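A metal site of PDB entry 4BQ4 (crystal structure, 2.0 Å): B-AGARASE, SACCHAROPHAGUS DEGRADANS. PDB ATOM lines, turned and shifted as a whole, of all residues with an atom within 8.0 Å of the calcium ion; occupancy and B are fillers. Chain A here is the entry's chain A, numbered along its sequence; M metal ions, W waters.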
ATOM      1  N   MET A   4      11.093  -1.754   5.336  1.00  0.00           N
ATOM      2  CA  MET A   4      10.414  -0.713   4.577  1.00  0.00           C
ATOM      3  C   MET A   4       9.885  -1.235   3.244  1.00  0.00           C
ATOM      4  O   MET A   4      10.606  -1.849   2.482  1.00  0.00           O
ATOM      5  CB  MET A   4      11.341   0.515   4.368  1.00  0.00           C
ATOM      6  CG  MET A   4      10.683   1.667   3.625  1.00  0.00           C
ATOM      7  SD  MET A   4       9.279   2.437   4.495  1.00  0.00           S
ATOM      8  CE  MET A   4      10.026   3.088   5.976  1.00  0.00           C
ATOM      9  N   PHE A   6       7.390   0.804   1.174  1.00  0.00           N
ATOM     10  CA  PHE A   6       7.198   1.961   0.306  1.00  0.00           C
ATOM     11  C   PHE A   6       7.386   3.237   1.130  1.00  0.00           C
ATOM     12  O   PHE A   6       6.591   3.527   2.045  1.00  0.00           O
ATOM     13  CB  PHE A   6       5.801   2.013  -0.350  1.00  0.00           C
ATOM     14  CG  PHE A   6       5.446   0.805  -1.186  1.00  0.00           C
ATOM     15  CD1 PHE A   6       4.837  -0.293  -0.622  1.00  0.00           C
ATOM     16  CD2 PHE A   6       5.675   0.797  -2.544  1.00  0.00           C
ATOM     17  CE1 PHE A   6       4.475  -1.405  -1.391  1.00  0.00           C
ATOM     18  CE2 PHE A   6       5.328  -0.303  -3.324  1.00  0.00           C
ATOM     19  CZ  PHE A   6       4.711  -1.418  -2.744  1.00  0.00           C
ATOM     20  N   ASP A   7       8.420   4.006   0.812  1.00  0.00           N
ATOM     21  CA  ASP A   7       8.566   5.327   1.420  1.00  0.00           C
ATOM     22  C   ASP A   7       8.339   6.441   0.411  1.00  0.00           C
ATOM     23  O   ASP A   7       8.454   7.609   0.767  1.00  0.00           O
ATOM     24  CB  ASP A   7       9.919   5.492   2.116  1.00  0.00           C
ATOM     25  CG  ASP A   7      11.092   5.325   1.164  1.00  0.00           C
ATOM     26  OD1 ASP A   7      10.922   5.306  -0.095  1.00  0.00           O
ATOM     27  OD2 ASP A   7      12.213   5.200   1.704  1.00  0.00           O
ATOM     28  N   PHE A   8       8.063   6.063  -0.833  1.00  0.00           N
ATOM     29  CA  PHE A   8       7.792   7.011  -1.925  1.00  0.00           C
ATOM     30  C   PHE A   8       8.878   8.108  -2.181  1.00  0.00           C
ATOM     31  O   PHE A   8       8.611   9.094  -2.914  1.00  0.00           O
ATOM     32  CB  PHE A   8       6.374   7.630  -1.747  1.00  0.00           C
ATOM     33  CG  PHE A   8       5.318   6.588  -1.533  1.00  0.00           C
ATOM     34  CD1 PHE A   8       4.888   5.803  -2.590  1.00  0.00           C
ATOM     35  CD2 PHE A   8       4.821   6.338  -0.250  1.00  0.00           C
ATOM     36  CE1 PHE A   8       3.951   4.794  -2.391  1.00  0.00           C
ATOM     37  CE2 PHE A   8       3.878   5.327  -0.044  1.00  0.00           C
ATOM     38  CZ  PHE A   8       3.429   4.572  -1.109  1.00  0.00           C
ATOM     39  N   GLU A   9      10.077   7.902  -1.625  1.00  0.00           N
ATOM     40  CA  GLU A   9      11.148   8.908  -1.654  1.00  0.00           C
ATOM     41  C   GLU A   9      11.781   8.988  -3.037  1.00  0.00           C
ATOM     42  O   GLU A   9      12.468   9.952  -3.351  1.00  0.00           O
ATOM     43  CB  GLU A   9      12.215   8.620  -0.588  1.00  0.00           C
ATOM     44  CG  GLU A   9      11.783   9.026   0.818  1.00  0.00           C
ATOM     45  CD  GLU A   9      11.396  10.499   0.927  1.00  0.00           C
ATOM     46  OE1 GLU A   9      12.067  11.357   0.318  1.00  0.00           O
ATOM     47  OE2 GLU A   9      10.394  10.811   1.619  1.00  0.00           O
ATOM     48  N   ASN A  10      11.500   7.989  -3.858  1.00  0.00           N
ATOM     49  CA  ASN A  10      11.993   7.952  -5.223  1.00  0.00           C
ATOM     50  C   ASN A  10      10.990   8.642  -6.147  1.00  0.00           C
ATOM     51  O   ASN A  10      11.109   8.562  -7.376  1.00  0.00           O
ATOM     52  CB  ASN A  10      12.297   6.504  -5.662  1.00  0.00           C
ATOM     53  CG  ASN A  10      11.025   5.654  -5.857  1.00  0.00           C
ATOM     54  OD1 ASN A  10       9.916   6.181  -5.960  1.00  0.00           O
ATOM     55  ND2 ASN A  10      11.206   4.331  -5.913  1.00  0.00           N
ATOM     56  N   ILE A  26       2.606  11.640  -6.043  1.00  0.00           N
ATOM     57  CA  ILE A  26       3.557  11.830  -4.958  1.00  0.00           C
ATOM     58  C   ILE A  26       3.654  13.326  -4.632  1.00  0.00           C
ATOM     59  O   ILE A  26       3.673  14.153  -5.527  1.00  0.00           O
ATOM     60  CB  ILE A  26       4.958  11.264  -5.306  1.00  0.00           C
ATOM     61  CG1 ILE A  26       4.854   9.869  -5.898  1.00  0.00           C
ATOM     62  CG2 ILE A  26       5.896  11.299  -4.086  1.00  0.00           C
ATOM     63  CD1 ILE A  26       4.069   8.862  -5.077  1.00  0.00           C
ATOM     64  N   GLU A  27       3.683  13.658  -3.348  1.00  0.00           N
ATOM     65  CA  GLU A  27       3.708  15.027  -2.914  1.00  0.00           C
ATOM     66  C   GLU A  27       4.570  15.138  -1.698  1.00  0.00           C
ATOM     67  O   GLU A  27       4.704  14.168  -0.949  1.00  0.00           O
ATOM     68  CB  GLU A  27       2.298  15.506  -2.541  1.00  0.00           C
ATOM     69  CG  GLU A  27       1.505  16.093  -3.686  1.00  0.00           C
ATOM     70  CD  GLU A  27       0.208  16.767  -3.232  1.00  0.00           C
ATOM     71  OE1 GLU A  27       0.013  16.999  -2.004  1.00  0.00           O
ATOM     72  OE2 GLU A  27      -0.615  17.074  -4.117  1.00  0.00           O
ATOM     73  N   TYR A  29       5.037  16.614   1.983  1.00  0.00           N
ATOM     74  CA  TYR A  29       4.139  16.955   3.074  1.00  0.00           C
ATOM     75  C   TYR A  29       4.999  16.855   4.344  1.00  0.00           C
ATOM     76  O   TYR A  29       6.120  16.370   4.285  1.00  0.00           O
ATOM     77  CB  TYR A  29       2.954  15.954   3.080  1.00  0.00           C
ATOM     78  CG  TYR A  29       3.369  14.640   3.687  1.00  0.00           C
ATOM     79  CD1 TYR A  29       4.120  13.702   2.939  1.00  0.00           C
ATOM     80  CD2 TYR A  29       3.064  14.360   5.010  1.00  0.00           C
ATOM     81  CE1 TYR A  29       4.541  12.522   3.542  1.00  0.00           C
ATOM     82  CE2 TYR A  29       3.478  13.199   5.599  1.00  0.00           C
ATOM     83  CZ  TYR A  29       4.208  12.277   4.877  1.00  0.00           C
ATOM     84  OH  TYR A  29       4.614  11.141   5.518  1.00  0.00           O
ATOM     85  N   GLY A  31       5.845  15.036   7.572  1.00  0.00           N
ATOM     86  CA  GLY A  31       5.583  13.737   8.143  1.00  0.00           C
ATOM     87  C   GLY A  31       5.486  13.753   9.645  1.00  0.00           C
ATOM     88  O   GLY A  31       5.487  14.817  10.288  1.00  0.00           O
ATOM     89  N   PRO A  36       9.936  17.496   6.174  1.00  0.00           N
ATOM     90  CA  PRO A  36       9.240  17.225   4.897  1.00  0.00           C
ATOM     91  C   PRO A  36       9.650  15.862   4.327  1.00  0.00           C
ATOM     92  O   PRO A  36      10.754  15.394   4.582  1.00  0.00           O
ATOM     93  CB  PRO A  36       9.710  18.359   3.961  1.00  0.00           C
ATOM     94  CG  PRO A  36      10.483  19.304   4.806  1.00  0.00           C
ATOM     95  CD  PRO A  36      10.945  18.564   6.032  1.00  0.00           C
ATOM     96  N   SER A  37       8.767  15.240   3.546  1.00  0.00           N
ATOM     97  CA  SER A  37       8.928  13.844   3.148  1.00  0.00           C
ATOM     98  C   SER A  37       8.095  13.656   1.886  1.00  0.00           C
ATOM     99  O   SER A  37       7.162  14.407   1.675  1.00  0.00           O
ATOM    100  CB  SER A  37       8.376  12.963   4.270  1.00  0.00           C
ATOM    101  OG  SER A  37       8.605  11.598   4.049  1.00  0.00           O
ATOM    102  N   LYS A  38       8.419  12.669   1.051  1.00  0.00           N
ATOM    103  CA  LYS A  38       7.542  12.233  -0.044  1.00  0.00           C
ATOM    104  C   LYS A  38       6.487  11.233   0.438  1.00  0.00           C
ATOM    105  O   LYS A  38       6.806  10.240   1.107  1.00  0.00           O
ATOM    106  CB  LYS A  38       8.355  11.627  -1.197  1.00  0.00           C
ATOM    107  CG  LYS A  38       9.228  12.640  -1.948  1.00  0.00           C
ATOM    108  CD  LYS A  38       8.344  13.726  -2.560  1.00  0.00           C
ATOM    109  CE  LYS A  38       9.131  14.851  -3.211  1.00  0.00           C
ATOM    110  NZ  LYS A  38      10.287  14.255  -3.925  1.00  0.00           N
ATOM    111  N   GLY A  39       5.236  11.485   0.096  1.00  0.00           N
ATOM    112  CA  GLY A  39       4.166  10.526   0.357  1.00  0.00           C
ATOM    113  C   GLY A  39       3.212  10.374  -0.812  1.00  0.00           C
ATOM    114  O   GLY A  39       3.151  11.227  -1.723  1.00  0.00           O
ATOM    115  N   LEU A  40       2.448   9.281  -0.781  1.00  0.00           N
ATOM    116  CA  LEU A  40       1.415   9.060  -1.769  1.00  0.00           C
ATOM    117  C   LEU A  40       0.099   9.798  -1.431  1.00  0.00           C
ATOM    118  O   LEU A  40      -0.565   9.554  -0.407  1.00  0.00           O
ATOM    119  CB  LEU A  40       1.195   7.549  -1.961  1.00  0.00           C
ATOM    120  CG  LEU A  40       0.060   7.210  -2.927  1.00  0.00           C
ATOM    121  CD1 LEU A  40       0.629   7.041  -4.313  1.00  0.00           C
ATOM    122  CD2 LEU A  40      -0.655   5.928  -2.527  1.00  0.00           C
ATOM    123  N   ASP A  75       1.693   5.117   7.564  1.00  0.00           N
ATOM    124  CA  ASP A  75       1.463   6.465   8.090  1.00  0.00           C
ATOM    125  C   ASP A  75       0.321   7.038   7.262  1.00  0.00           C
ATOM    126  O   ASP A  75       0.386   7.007   6.055  1.00  0.00           O
ATOM    127  CB  ASP A  75       2.690   7.356   7.951  1.00  0.00           C
ATOM    128  CG  ASP A  75       3.859   6.942   8.862  1.00  0.00           C
ATOM    129  OD1 ASP A  75       3.760   6.031   9.712  1.00  0.00           O
ATOM    130  OD2 ASP A  75       4.926   7.568   8.678  1.00  0.00           O
ATOM    131  N   ILE A 184      -0.531   8.798   2.299  1.00  0.00           N
ATOM    132  CA  ILE A 184      -0.051   7.546   2.855  1.00  0.00           C
ATOM    133  C   ILE A 184       1.470   7.572   2.697  1.00  0.00           C
ATOM    134  O   ILE A 184       1.952   8.080   1.680  1.00  0.00           O
ATOM    135  CB  ILE A 184      -0.625   6.344   2.080  1.00  0.00           C
ATOM    136  CG1 ILE A 184      -2.153   6.262   2.324  1.00  0.00           C
ATOM    137  CG2 ILE A 184       0.017   5.035   2.544  1.00  0.00           C
ATOM    138  CD1 ILE A 184      -2.894   5.540   1.193  1.00  0.00           C
ATOM    139  N   ASP A 185       2.202   7.051   3.668  1.00  0.00           N
ATOM    140  CA  ASP A 185       3.681   7.054   3.613  1.00  0.00           C
ATOM    141  C   ASP A 185       4.224   5.944   4.483  1.00  0.00           C
ATOM    142  O   ASP A 185       3.539   5.451   5.421  1.00  0.00           O
ATOM    143  CB  ASP A 185       4.227   8.395   4.126  1.00  0.00           C
ATOM    144  CG  ASP A 185       5.685   8.639   3.723  1.00  0.00           C
ATOM    145  OD1 ASP A 185       6.218   7.856   2.891  1.00  0.00           O
ATOM    146  OD2 ASP A 185       6.285   9.617   4.222  1.00  0.00           O
ATOM    147  N   ASN A 186       5.459   5.538   4.196  1.00  0.00           N
ATOM    148  CA  ASN A 186       6.197   4.618   5.080  1.00  0.00           C
ATOM    149  C   ASN A 186       5.460   3.321   5.344  1.00  0.00           C
ATOM    150  O   ASN A 186       5.226   2.930   6.491  1.00  0.00           O
ATOM    151  CB  ASN A 186       6.554   5.327   6.386  1.00  0.00           C
ATOM    152  CG  ASN A 186       7.405   6.575   6.149  1.00  0.00           C
ATOM    153  OD1 ASN A 186       8.247   6.619   5.231  1.00  0.00           O
ATOM    154  ND2 ASN A 186       7.164   7.608   6.955  1.00  0.00           N
ATOM    155  N   ILE A 187       5.035   2.690   4.261  1.00  0.00           N
ATOM    156  CA  ILE A 187       4.394   1.396   4.382  1.00  0.00           C
ATOM    157  C   ILE A 187       5.503   0.415   4.717  1.00  0.00           C
ATOM    158  O   ILE A 187       6.484   0.296   3.974  1.00  0.00           O
ATOM    159  CB  ILE A 187       3.654   0.991   3.104  1.00  0.00           C
ATOM    160  CG1 ILE A 187       2.646   2.085   2.705  1.00  0.00           C
ATOM    161  CG2 ILE A 187       2.982  -0.372   3.275  1.00  0.00           C
ATOM    162  CD1 ILE A 187       1.897   1.822   1.414  1.00  0.00           C
HETATM  163 CA    CA M   1       8.417   9.266   2.430  1.00  0.00          CA
HETATM  164  O   HOH W   1      10.022   8.350   4.201  1.00  0.00           O
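The side-chain carboxylate (OD1) of Asp 185 lies close to the side-chain amide oxygen (OD1) of Asn 186 (3.3 Å).
OD2 of Asp 185 lies close to OH of Tyr 29 (2.6 Å).
O of Asp 185 is in hydrogen-bond range of N of Asp 75 (2.8 Å).
The backbone NH (N) of Ser 37 is in hydrogen-bond range of the backbone carbonyl oxygen (O) of Tyr 29, 3.0 Å away.
N of Asn 186 is in hydrogen-bond range of O of Phe 6.
OD2 of Asp 75 is in hydrogen-bond range of ND2 of Asn 186 (2.8 Å).
Merely in contact with the calcium ion: Asn 186.
Along chain A the residues within 4 Å of the calcium ion span positions 7 to 186.
The nearest printed residue that does not touch the calcium ion is Gly 39 (4.5 Å).
O of Lys 38 binds the calcium ion, at 2.3 Å.
O of Asp 7 is bound to the calcium ion (2.3 Å).
The calcium ion is bound by water W1.
OE2 of Glu 9 binds the calcium ion, at 2.6 Å.
The side-chain carboxylate (OD1) of Asp 185 binds the calcium ion, at 2.7 Å.
The calcium ion is bound by OD2 of Asp 185 (2.8 Å).
The side-chain hydroxyl (OG) of Ser 37 binds the calcium ion, 2.8 Å away.
The calcium ion has seven donor atoms within binding distance.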
